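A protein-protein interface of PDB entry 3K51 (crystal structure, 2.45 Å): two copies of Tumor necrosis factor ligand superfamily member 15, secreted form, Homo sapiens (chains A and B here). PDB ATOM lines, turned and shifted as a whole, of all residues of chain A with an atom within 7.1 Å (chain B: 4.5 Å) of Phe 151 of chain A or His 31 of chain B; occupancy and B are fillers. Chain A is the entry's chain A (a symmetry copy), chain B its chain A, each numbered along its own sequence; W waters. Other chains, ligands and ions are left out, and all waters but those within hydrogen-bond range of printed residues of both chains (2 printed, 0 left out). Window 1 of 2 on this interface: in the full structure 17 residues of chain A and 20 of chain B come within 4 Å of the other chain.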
ATOM      1  N   GLY A  78     -22.802 -11.752  14.497  1.00  0.00           N
ATOM      2  CA  GLY A  78     -21.744 -12.645  14.934  1.00  0.00           C
ATOM      3  C   GLY A  78     -21.567 -13.820  13.995  1.00  0.00           C
ATOM      4  O   GLY A  78     -22.220 -13.898  12.947  1.00  0.00           O
ATOM      5  N   ASP A  79     -20.685 -14.737  14.373  1.00  0.00           N
ATOM      6  CA  ASP A  79     -20.440 -15.938  13.598  1.00  0.00           C
ATOM      7  C   ASP A  79     -21.340 -17.076  14.050  1.00  0.00           C
ATOM      8  O   ASP A  79     -21.407 -17.396  15.247  1.00  0.00           O
ATOM      9  CB  ASP A  79     -18.976 -16.349  13.708  1.00  0.00           C
ATOM     10  CG  ASP A  79     -18.033 -15.279  13.189  1.00  0.00           C
ATOM     11  OD1 ASP A  79     -18.395 -14.585  12.209  1.00  0.00           O
ATOM     12  OD2 ASP A  79     -16.935 -15.125  13.762  1.00  0.00           O
ATOM     13  N   TYR A  80     -22.035 -17.681  13.087  1.00  0.00           N
ATOM     14  CA  TYR A  80     -22.978 -18.758  13.357  1.00  0.00           C
ATOM     15  C   TYR A  80     -22.553 -20.040  12.654  1.00  0.00           C
ATOM     16  O   TYR A  80     -22.047 -20.007  11.532  1.00  0.00           O
ATOM     17  CB  TYR A  80     -24.380 -18.373  12.867  1.00  0.00           C
ATOM     18  CG  TYR A  80     -25.071 -17.336  13.704  1.00  0.00           C
ATOM     19  CD1 TYR A  80     -26.096 -17.688  14.579  1.00  0.00           C
ATOM     20  CD2 TYR A  80     -24.710 -15.991  13.617  1.00  0.00           C
ATOM     21  CE1 TYR A  80     -26.739 -16.733  15.348  1.00  0.00           C
ATOM     22  CE2 TYR A  80     -25.343 -15.030  14.381  1.00  0.00           C
ATOM     23  CZ  TYR A  80     -26.354 -15.404  15.248  1.00  0.00           C
ATOM     24  OH  TYR A  80     -26.982 -14.450  16.008  1.00  0.00           O
ATOM     25  N   PHE A  81     -22.786 -21.171  13.302  1.00  0.00           N
ATOM     26  CA  PHE A  81     -22.795 -22.430  12.600  1.00  0.00           C
ATOM     27  C   PHE A  81     -24.226 -22.758  12.172  1.00  0.00           C
ATOM     28  O   PHE A  81     -25.147 -22.728  12.987  1.00  0.00           O
ATOM     29  CB  PHE A  81     -22.222 -23.554  13.470  1.00  0.00           C
ATOM     30  CG  PHE A  81     -21.942 -24.820  12.709  1.00  0.00           C
ATOM     31  CD1 PHE A  81     -20.791 -24.947  11.953  1.00  0.00           C
ATOM     32  CD2 PHE A  81     -22.851 -25.867  12.717  1.00  0.00           C
ATOM     33  CE1 PHE A  81     -20.537 -26.112  11.238  1.00  0.00           C
ATOM     34  CE2 PHE A  81     -22.605 -27.025  11.998  1.00  0.00           C
ATOM     35  CZ  PHE A  81     -21.446 -27.145  11.261  1.00  0.00           C
ATOM     36  N   ILE A  82     -24.401 -23.045  10.888  1.00  0.00           N
ATOM     37  CA  ILE A  82     -25.711 -23.360  10.314  1.00  0.00           C
ATOM     38  C   ILE A  82     -25.670 -24.735   9.656  1.00  0.00           C
ATOM     39  O   ILE A  82     -24.710 -25.060   8.960  1.00  0.00           O
ATOM     40  CB  ILE A  82     -26.104 -22.330   9.230  1.00  0.00           C
ATOM     41  CG1 ILE A  82     -25.913 -20.901   9.746  1.00  0.00           C
ATOM     42  CG2 ILE A  82     -27.532 -22.551   8.769  1.00  0.00           C
ATOM     43  CD1 ILE A  82     -25.971 -19.850   8.654  1.00  0.00           C
ATOM     44  N   ILE A 114     -28.986 -23.443   1.334  1.00  0.00           N
ATOM     45  CA  ILE A 114     -29.273 -22.586   2.470  1.00  0.00           C
ATOM     46  C   ILE A 114     -28.995 -21.134   2.108  1.00  0.00           C
ATOM     47  O   ILE A 114     -27.899 -20.785   1.662  1.00  0.00           O
ATOM     48  CB  ILE A 114     -28.494 -23.004   3.725  1.00  0.00           C
ATOM     49  CG1 ILE A 114     -28.863 -24.441   4.116  1.00  0.00           C
ATOM     50  CG2 ILE A 114     -28.792 -22.048   4.884  1.00  0.00           C
ATOM     51  CD1 ILE A 114     -28.245 -24.898   5.422  1.00  0.00           C
ATOM     52  N   LYS A 116     -29.420 -16.816   2.485  1.00  0.00           N
ATOM     53  CA  LYS A 116     -29.461 -15.680   3.381  1.00  0.00           C
ATOM     54  C   LYS A 116     -30.149 -14.489   2.714  1.00  0.00           C
ATOM     55  O   LYS A 116     -29.695 -13.994   1.686  1.00  0.00           O
ATOM     56  CB  LYS A 116     -28.044 -15.297   3.814  1.00  0.00           C
ATOM     57  CG  LYS A 116     -27.979 -14.102   4.750  1.00  0.00           C
ATOM     58  CD  LYS A 116     -26.539 -13.735   5.074  1.00  0.00           C
ATOM     59  CE  LYS A 116     -25.931 -12.864   3.998  1.00  0.00           C
ATOM     60  NZ  LYS A 116     -24.444 -12.771   4.140  1.00  0.00           N
ATOM     61  N   GLN A 126     -26.494 -17.334  -1.584  1.00  0.00           N
ATOM     62  CA  GLN A 126     -26.428 -18.778  -1.399  1.00  0.00           C
ATOM     63  C   GLN A 126     -25.219 -19.138  -0.537  1.00  0.00           C
ATOM     64  O   GLN A 126     -24.078 -19.065  -0.993  1.00  0.00           O
ATOM     65  CB  GLN A 126     -26.330 -19.485  -2.752  1.00  0.00           C
ATOM     66  CG  GLN A 126     -27.005 -18.739  -3.897  1.00  0.00           C
ATOM     67  CD  GLN A 126     -28.365 -19.310  -4.253  1.00  0.00           C
ATOM     68  OE1 GLN A 126     -28.478 -20.466  -4.668  1.00  0.00           O
ATOM     69  NE2 GLN A 126     -29.406 -18.492  -4.116  1.00  0.00           N
ATOM     70  N   LEU A 127     -25.475 -19.521   0.710  1.00  0.00           N
ATOM     71  CA  LEU A 127     -24.398 -19.847   1.645  1.00  0.00           C
ATOM     72  C   LEU A 127     -23.871 -21.268   1.447  1.00  0.00           C
ATOM     73  O   LEU A 127     -22.663 -21.496   1.443  1.00  0.00           O
ATOM     74  CB  LEU A 127     -24.869 -19.660   3.092  1.00  0.00           C
ATOM     75  CG  LEU A 127     -25.448 -18.295   3.467  1.00  0.00           C
ATOM     76  CD1 LEU A 127     -26.012 -18.325   4.888  1.00  0.00           C
ATOM     77  CD2 LEU A 127     -24.398 -17.179   3.314  1.00  0.00           C
ATOM     78  N   LEU A 128     -24.789 -22.216   1.279  1.00  0.00           N
ATOM     79  CA  LEU A 128     -24.438 -23.631   1.202  1.00  0.00           C
ATOM     80  C   LEU A 128     -25.288 -24.324   0.158  1.00  0.00           C
ATOM     81  O   LEU A 128     -26.497 -24.122   0.111  1.00  0.00           O
ATOM     82  CB  LEU A 128     -24.679 -24.304   2.549  1.00  0.00           C
ATOM     83  CG  LEU A 128     -23.742 -23.941   3.688  1.00  0.00           C
ATOM     84  CD1 LEU A 128     -24.278 -24.475   5.007  1.00  0.00           C
ATOM     85  CD2 LEU A 128     -22.365 -24.482   3.404  1.00  0.00           C
ATOM     86  N   GLY A 148     -23.453 -28.263   6.590  1.00  0.00           N
ATOM     87  CA  GLY A 148     -23.159 -27.473   7.776  1.00  0.00           C
ATOM     88  C   GLY A 148     -21.905 -26.643   7.592  1.00  0.00           C
ATOM     89  O   GLY A 148     -20.903 -27.131   7.077  1.00  0.00           O
ATOM     90  N   ALA A 149     -21.957 -25.381   8.005  1.00  0.00           N
ATOM     91  CA  ALA A 149     -20.788 -24.518   7.929  1.00  0.00           C
ATOM     92  C   ALA A 149     -20.960 -23.253   8.744  1.00  0.00           C
ATOM     93  O   ALA A 149     -22.052 -22.956   9.226  1.00  0.00           O
ATOM     94  CB  ALA A 149     -20.470 -24.176   6.479  1.00  0.00           C
ATOM     95  N   MET A 150     -19.871 -22.501   8.877  1.00  0.00           N
ATOM     96  CA  MET A 150     -19.852 -21.294   9.681  1.00  0.00           C
ATOM     97  C   MET A 150     -19.904 -20.029   8.809  1.00  0.00           C
ATOM     98  O   MET A 150     -19.250 -19.950   7.774  1.00  0.00           O
ATOM     99  CB  MET A 150     -18.606 -21.282  10.563  1.00  0.00           C
ATOM    100  CG  MET A 150     -18.309 -19.960  11.224  1.00  0.00           C
ATOM    101  SD  MET A 150     -16.756 -20.018  12.151  1.00  0.00           S
ATOM    102  CE  MET A 150     -15.595 -20.427  10.848  1.00  0.00           C
ATOM    103  N   PHE A 151     -20.683 -19.045   9.245  1.00  0.00           N
ATOM    104  CA  PHE A 151     -20.861 -17.821   8.486  1.00  0.00           C
ATOM    105  C   PHE A 151     -20.980 -16.614   9.401  1.00  0.00           C
ATOM    106  O   PHE A 151     -21.555 -16.700  10.490  1.00  0.00           O
ATOM    107  CB  PHE A 151     -22.109 -17.924   7.596  1.00  0.00           C
ATOM    108  CG  PHE A 151     -22.033 -19.020   6.572  1.00  0.00           C
ATOM    109  CD1 PHE A 151     -21.398 -18.812   5.358  1.00  0.00           C
ATOM    110  CD2 PHE A 151     -22.575 -20.267   6.831  1.00  0.00           C
ATOM    111  CE1 PHE A 151     -21.310 -19.818   4.423  1.00  0.00           C
ATOM    112  CE2 PHE A 151     -22.494 -21.281   5.896  1.00  0.00           C
ATOM    113  CZ  PHE A 151     -21.860 -21.056   4.690  1.00  0.00           C
ATOM    114  N   SER A 152     -20.412 -15.494   8.963  1.00  0.00           N
ATOM    115  CA  SER A 152     -20.617 -14.223   9.639  1.00  0.00           C
ATOM    116  C   SER A 152     -21.961 -13.627   9.240  1.00  0.00           C
ATOM    117  O   SER A 152     -22.202 -13.341   8.069  1.00  0.00           O
ATOM    118  CB  SER A 152     -19.478 -13.247   9.320  1.00  0.00           C
ATOM    119  OG  SER A 152     -18.334 -13.510  10.126  1.00  0.00           O
ATOM    120  N   LEU A 153     -22.838 -13.454  10.220  1.00  0.00           N
ATOM    121  CA  LEU A 153     -24.189 -12.954   9.954  1.00  0.00           C
ATOM    122  C   LEU A 153     -24.468 -11.665  10.717  1.00  0.00           C
ATOM    123  O   LEU A 153     -23.793 -11.355  11.702  1.00  0.00           O
ATOM    124  CB  LEU A 153     -25.241 -14.017  10.312  1.00  0.00           C
ATOM    125  CG  LEU A 153     -25.125 -15.362   9.587  1.00  0.00           C
ATOM    126  CD1 LEU A 153     -26.114 -16.379  10.159  1.00  0.00           C
ATOM    127  CD2 LEU A 153     -25.326 -15.199   8.076  1.00  0.00           C
ATOM    128  N   GLN A 154     -25.471 -10.926  10.267  1.00  0.00           N
ATOM    129  CA  GLN A 154     -25.824  -9.656  10.888  1.00  0.00           C
ATOM    130  C   GLN A 154     -27.214  -9.700  11.479  1.00  0.00           C
ATOM    131  O   GLN A 154     -28.090 -10.411  10.987  1.00  0.00           O
ATOM    132  CB  GLN A 154     -25.727  -8.515   9.877  1.00  0.00           C
ATOM    133  CG  GLN A 154     -24.486  -8.578   8.998  1.00  0.00           C
ATOM    134  CD  GLN A 154     -23.811  -7.236   8.855  1.00  0.00           C
ATOM    135  OE1 GLN A 154     -23.758  -6.668   7.763  1.00  0.00           O
ATOM    136  NE2 GLN A 154     -23.290  -6.714   9.963  1.00  0.00           N
ATOM    137  N   LEU A 159     -32.591 -16.553   7.383  1.00  0.00           N
ATOM    138  CA  LEU A 159     -32.092 -17.779   6.784  1.00  0.00           C
ATOM    139  C   LEU A 159     -33.243 -18.680   6.374  1.00  0.00           C
ATOM    140  O   LEU A 159     -34.209 -18.840   7.116  1.00  0.00           O
ATOM    141  CB  LEU A 159     -31.175 -18.524   7.759  1.00  0.00           C
ATOM    142  CG  LEU A 159     -29.936 -17.793   8.277  1.00  0.00           C
ATOM    143  CD1 LEU A 159     -29.303 -18.564   9.436  1.00  0.00           C
ATOM    144  CD2 LEU A 159     -28.930 -17.570   7.162  1.00  0.00           C
ATOM    145  N   LEU A 184     -21.735 -18.945  17.728  1.00  0.00           N
ATOM    146  CA  LEU A 184     -20.547 -19.530  18.307  1.00  0.00           C
ATOM    147  C   LEU A 184     -20.080 -18.726  19.525  1.00  0.00           C
ATOM    148  O   LEU A 184     -19.864 -17.509  19.451  1.00  0.00           O
ATOM    149  CB  LEU A 184     -19.443 -19.624  17.262  1.00  0.00           C
ATOM    150  CG  LEU A 184     -19.817 -20.449  16.023  1.00  0.00           C
ATOM    151  CD1 LEU A 184     -18.679 -20.484  15.017  1.00  0.00           C
ATOM    152  CD2 LEU A 184     -20.234 -21.860  16.422  1.00  0.00           C
ATOM    153  OXT LEU A 184     -19.937 -19.275  20.623  1.00  0.00           O
ATOM    154  N   ALA B  30     -12.107 -19.743  10.696  1.00  0.00           N
ATOM    155  CA  ALA B  30     -11.937 -19.543   9.272  1.00  0.00           C
ATOM    156  C   ALA B  30     -12.950 -20.352   8.494  1.00  0.00           C
ATOM    157  O   ALA B  30     -13.249 -21.489   8.840  1.00  0.00           O
ATOM    158  CB  ALA B  30     -10.520 -19.904   8.841  1.00  0.00           C
ATOM    159  N   HIS B  31     -13.496 -19.749   7.453  1.00  0.00           N
ATOM    160  CA  HIS B  31     -14.271 -20.477   6.479  1.00  0.00           C
ATOM    161  C   HIS B  31     -13.680 -20.210   5.108  1.00  0.00           C
ATOM    162  O   HIS B  31     -13.622 -19.066   4.664  1.00  0.00           O
ATOM    163  CB  HIS B  31     -15.737 -20.041   6.526  1.00  0.00           C
ATOM    164  CG  HIS B  31     -16.591 -20.696   5.490  1.00  0.00           C
ATOM    165  ND1 HIS B  31     -17.036 -21.996   5.606  1.00  0.00           N
ATOM    166  CD2 HIS B  31     -17.069 -20.237   4.310  1.00  0.00           C
ATOM    167  CE1 HIS B  31     -17.761 -22.306   4.545  1.00  0.00           C
ATOM    168  NE2 HIS B  31     -17.797 -21.256   3.744  1.00  0.00           N
ATOM    169  N   LEU B  32     -13.210 -21.265   4.453  1.00  0.00           N
ATOM    170  CA  LEU B  32     -12.531 -21.129   3.171  1.00  0.00           C
ATOM    171  C   LEU B  32     -13.386 -21.694   2.048  1.00  0.00           C
ATOM    172  O   LEU B  32     -14.117 -22.655   2.241  1.00  0.00           O
ATOM    173  CB  LEU B  32     -11.180 -21.848   3.203  1.00  0.00           C
ATOM    174  CG  LEU B  32     -10.255 -21.597   4.391  1.00  0.00           C
ATOM    175  CD1 LEU B  32      -8.945 -22.378   4.211  1.00  0.00           C
ATOM    176  CD2 LEU B  32      -9.979 -20.101   4.573  1.00  0.00           C
ATOM    177  N   THR B  33     -13.273 -21.104   0.868  1.00  0.00           N
ATOM    178  CA  THR B  33     -14.079 -21.525  -0.264  1.00  0.00           C
ATOM    179  C   THR B  33     -13.215 -21.907  -1.463  1.00  0.00           C
ATOM    180  O   THR B  33     -12.079 -21.462  -1.589  1.00  0.00           O
ATOM    181  CB  THR B  33     -15.071 -20.436  -0.677  1.00  0.00           C
ATOM    182  OG1 THR B  33     -14.359 -19.230  -0.966  1.00  0.00           O
ATOM    183  CG2 THR B  33     -16.069 -20.170   0.446  1.00  0.00           C
ATOM    184  N   LEU B  58     -17.771 -15.309   0.740  1.00  0.00           N
ATOM    185  CA  LEU B  58     -18.135 -15.885   2.026  1.00  0.00           C
ATOM    186  C   LEU B  58     -16.912 -16.362   2.812  1.00  0.00           C
ATOM    187  O   LEU B  58     -17.041 -16.868   3.926  1.00  0.00           O
ATOM    188  CB  LEU B  58     -19.109 -17.044   1.821  1.00  0.00           C
ATOM    189  CG  LEU B  58     -20.419 -16.661   1.130  1.00  0.00           C
ATOM    190  CD1 LEU B  58     -21.195 -17.897   0.719  1.00  0.00           C
ATOM    191  CD2 LEU B  58     -21.253 -15.768   2.038  1.00  0.00           C
ATOM    192  N   ALA B  59     -15.733 -16.205   2.226  1.00  0.00           N
ATOM    193  CA  ALA B  59     -14.511 -16.694   2.842  1.00  0.00           C
ATOM    194  C   ALA B  59     -13.944 -15.657   3.783  1.00  0.00           C
ATOM    195  O   ALA B  59     -13.957 -14.461   3.486  1.00  0.00           O
ATOM    196  CB  ALA B  59     -13.491 -17.062   1.785  1.00  0.00           C
ATOM    197  N   PHE B  60     -13.452 -16.113   4.926  1.00  0.00           N
ATOM    198  CA  PHE B  60     -12.857 -15.225   5.903  1.00  0.00           C
ATOM    199  C   PHE B  60     -11.946 -16.002   6.831  1.00  0.00           C
ATOM    200  O   PHE B  60     -12.093 -17.212   6.987  1.00  0.00           O
ATOM    201  CB  PHE B  60     -13.945 -14.497   6.714  1.00  0.00           C
ATOM    202  CG  PHE B  60     -14.617 -15.362   7.752  1.00  0.00           C
ATOM    203  CD1 PHE B  60     -14.072 -15.496   9.028  1.00  0.00           C
ATOM    204  CD2 PHE B  60     -15.790 -16.037   7.457  1.00  0.00           C
ATOM    205  CE1 PHE B  60     -14.686 -16.297   9.985  1.00  0.00           C
ATOM    206  CE2 PHE B  60     -16.408 -16.838   8.410  1.00  0.00           C
ATOM    207  CZ  PHE B  60     -15.854 -16.963   9.678  1.00  0.00           C
ATOM    208  N   TYR B  83     -14.571 -28.898   9.429  1.00  0.00           N
ATOM    209  CA  TYR B  83     -15.516 -29.415   8.456  1.00  0.00           C
ATOM    210  C   TYR B  83     -15.061 -29.131   7.034  1.00  0.00           C
ATOM    211  O   TYR B  83     -14.262 -28.217   6.788  1.00  0.00           O
ATOM    212  CB  TYR B  83     -16.902 -28.818   8.686  1.00  0.00           C
ATOM    213  CG  TYR B  83     -16.939 -27.307   8.565  1.00  0.00           C
ATOM    214  CD1 TYR B  83     -17.175 -26.691   7.332  1.00  0.00           C
ATOM    215  CD2 TYR B  83     -16.730 -26.495   9.679  1.00  0.00           C
ATOM    216  CE1 TYR B  83     -17.197 -25.309   7.214  1.00  0.00           C
ATOM    217  CE2 TYR B  83     -16.748 -25.109   9.570  1.00  0.00           C
ATOM    218  CZ  TYR B  83     -16.988 -24.522   8.337  1.00  0.00           C
ATOM    219  OH  TYR B  83     -17.011 -23.154   8.227  1.00  0.00           O
ATOM    220  N   PHE B 178     -15.970 -26.212   0.137  1.00  0.00           N
ATOM    221  CA  PHE B 178     -15.526 -25.305   1.193  1.00  0.00           C
ATOM    222  C   PHE B 178     -14.843 -26.047   2.335  1.00  0.00           C
ATOM    223  O   PHE B 178     -14.873 -27.274   2.397  1.00  0.00           O
ATOM    224  CB  PHE B 178     -16.710 -24.480   1.730  1.00  0.00           C
ATOM    225  CG  PHE B 178     -17.899 -25.316   2.132  1.00  0.00           C
ATOM    226  CD1 PHE B 178     -17.927 -25.965   3.361  1.00  0.00           C
ATOM    227  CD2 PHE B 178     -18.979 -25.469   1.274  1.00  0.00           C
ATOM    228  CE1 PHE B 178     -19.012 -26.735   3.732  1.00  0.00           C
ATOM    229  CE2 PHE B 178     -20.066 -26.244   1.640  1.00  0.00           C
ATOM    230  CZ  PHE B 178     -20.082 -26.878   2.875  1.00  0.00           C
ATOM    231  N   PHE B 179     -14.256 -25.286   3.251  1.00  0.00           N
ATOM    232  CA  PHE B 179     -13.387 -25.836   4.281  1.00  0.00           C
ATOM    233  C   PHE B 179     -13.287 -24.831   5.414  1.00  0.00           C
ATOM    234  O   PHE B 179     -12.961 -23.669   5.189  1.00  0.00           O
ATOM    235  CB  PHE B 179     -11.999 -26.094   3.686  1.00  0.00           C
ATOM    236  CG  PHE B 179     -10.956 -26.515   4.697  1.00  0.00           C
ATOM    237  CD1 PHE B 179     -11.273 -27.368   5.737  1.00  0.00           C
ATOM    238  CD2 PHE B 179      -9.633 -26.119   4.544  1.00  0.00           C
ATOM    239  CE1 PHE B 179     -10.294 -27.783   6.644  1.00  0.00           C
ATOM    240  CE2 PHE B 179      -8.659 -26.527   5.438  1.00  0.00           C
ATOM    241  CZ  PHE B 179      -8.990 -27.360   6.490  1.00  0.00           C
ATOM    242  N   GLY B 180     -13.577 -25.272   6.632  1.00  0.00           N
ATOM    243  CA  GLY B 180     -13.557 -24.371   7.769  1.00  0.00           C
ATOM    244  C   GLY B 180     -13.151 -25.019   9.068  1.00  0.00           C
ATOM    245  O   GLY B 180     -13.078 -26.246   9.169  1.00  0.00           O
HETATM  246  O   HOH W   1     -19.512 -21.541   1.530  1.00  0.00           O
HETATM  247  O   HOH W   2     -18.475 -17.702   6.086  1.00  0.00           O
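The backbone NH (N) of Met 150 of chain A lies within hydrogen-bond range of the side-chain hydroxyl (OH) of Tyr 83 of chain B.
The side-chain hydroxyl (OH) of Tyr 83 of chain B is in hydrogen-bond range of a ring nitrogen (ND1) of His 31 of chain B, at 2.9 Å. O of Ile 114 of chain A sits at hydrogen-bond distance from N of Leu 127 of chain A, at 2.9 Å. The backbone carbonyl oxygen (O) of Ala 149 of chain A sits at hydrogen-bond distance from the backbone NH (N) of Ile 82 of chain A, at 2.9 Å. The backbone NH (N) of His 31 of chain B is in hydrogen-bond range of the backbone carbonyl oxygen (O) of Phe 60 of chain B, 2.9 Å away. The backbone NH (N) of Gly 180 of chain B sits at hydrogen-bond distance from the backbone carbonyl oxygen (O) of Tyr 83 of chain B (3.0 Å). O of Phe 151 of chain A lies within hydrogen-bond range of N of Tyr 80 of chain A, at 2.8 Å.
Among the printed residues, pairs that only touch across the chains: Met 150 of chain A with Ala 30 of chain B (3.3 Å), Leu 128 of chain A with Phe 178 of chain B (3.4 Å), Ala 149 of chain A with Tyr 83 of chain B (3.5 Å), Gln 126 of chain A with Leu 58 of chain B (3.6 Å), Met 150 of chain A with His 31 of chain B (3.6 Å), Met 150 of chain A with Phe 60 of chain B (3.7 Å), Leu 127 of chain A with Leu 58 of chain B (3.7 Å), Gly 148 of chain A with Tyr 83 of chain B (3.8 Å), Ala 149 of chain A with His 31 of chain B (3.8 Å), Phe 151 of chain A with His 31 of chain B (3.9 Å) and Gly 148 of chain A with Phe 178 of chain B (3.9 Å).
Of chain B, only His 31 comes within 4 Å of Phe 151 of chain A. Of chain A, only Ala 149, Met 150 and Phe 151 come within 4 Å of His 31 of chain B. Printed residues of chain B within 4 Å of Gln 126 of chain A: Leu 58. Printed residues of chain B within 4 Å of Ala 149 of chain A: His 31 (3.8 Å) and Tyr 83 (3.5 Å). Phe 179 of chain B touches none of the printed residues of chain A. Phe 81 of chain A touches none of the printed residues of chain B. The nearest residue of chain A that does not touch His 31 of chain B is Leu 128 of chain A (5.2 Å). The nearest printed residue of chain A that does not touch Ala 30 of chain B is Asp 79 of chain A (7.4 Å).
Of the 19 printed residues of chain A, 7 touch a printed residue of chain B. Hydrophobic or aromatic side chains of chain A within 4 Å of the printed part of chain B: Leu 127, Leu 128, Ala 149, Met 150 and Phe 151. Among the printed residues, no Asp or Glu carboxylate lies within 4 Å of a Lys or Arg side-chain nitrogen of the other chain.
No position is printed for both chains.
Water W2 bridges O of Leu 58 of chain B (2.7 Å) and O of Met 150 of chain A (2.9 Å). Water W1 lies within hydrogen-bond range of a ring nitrogen (NE2) of His 31 of chain B and the backbone carbonyl oxygen (O) of Leu 127 of chain A.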
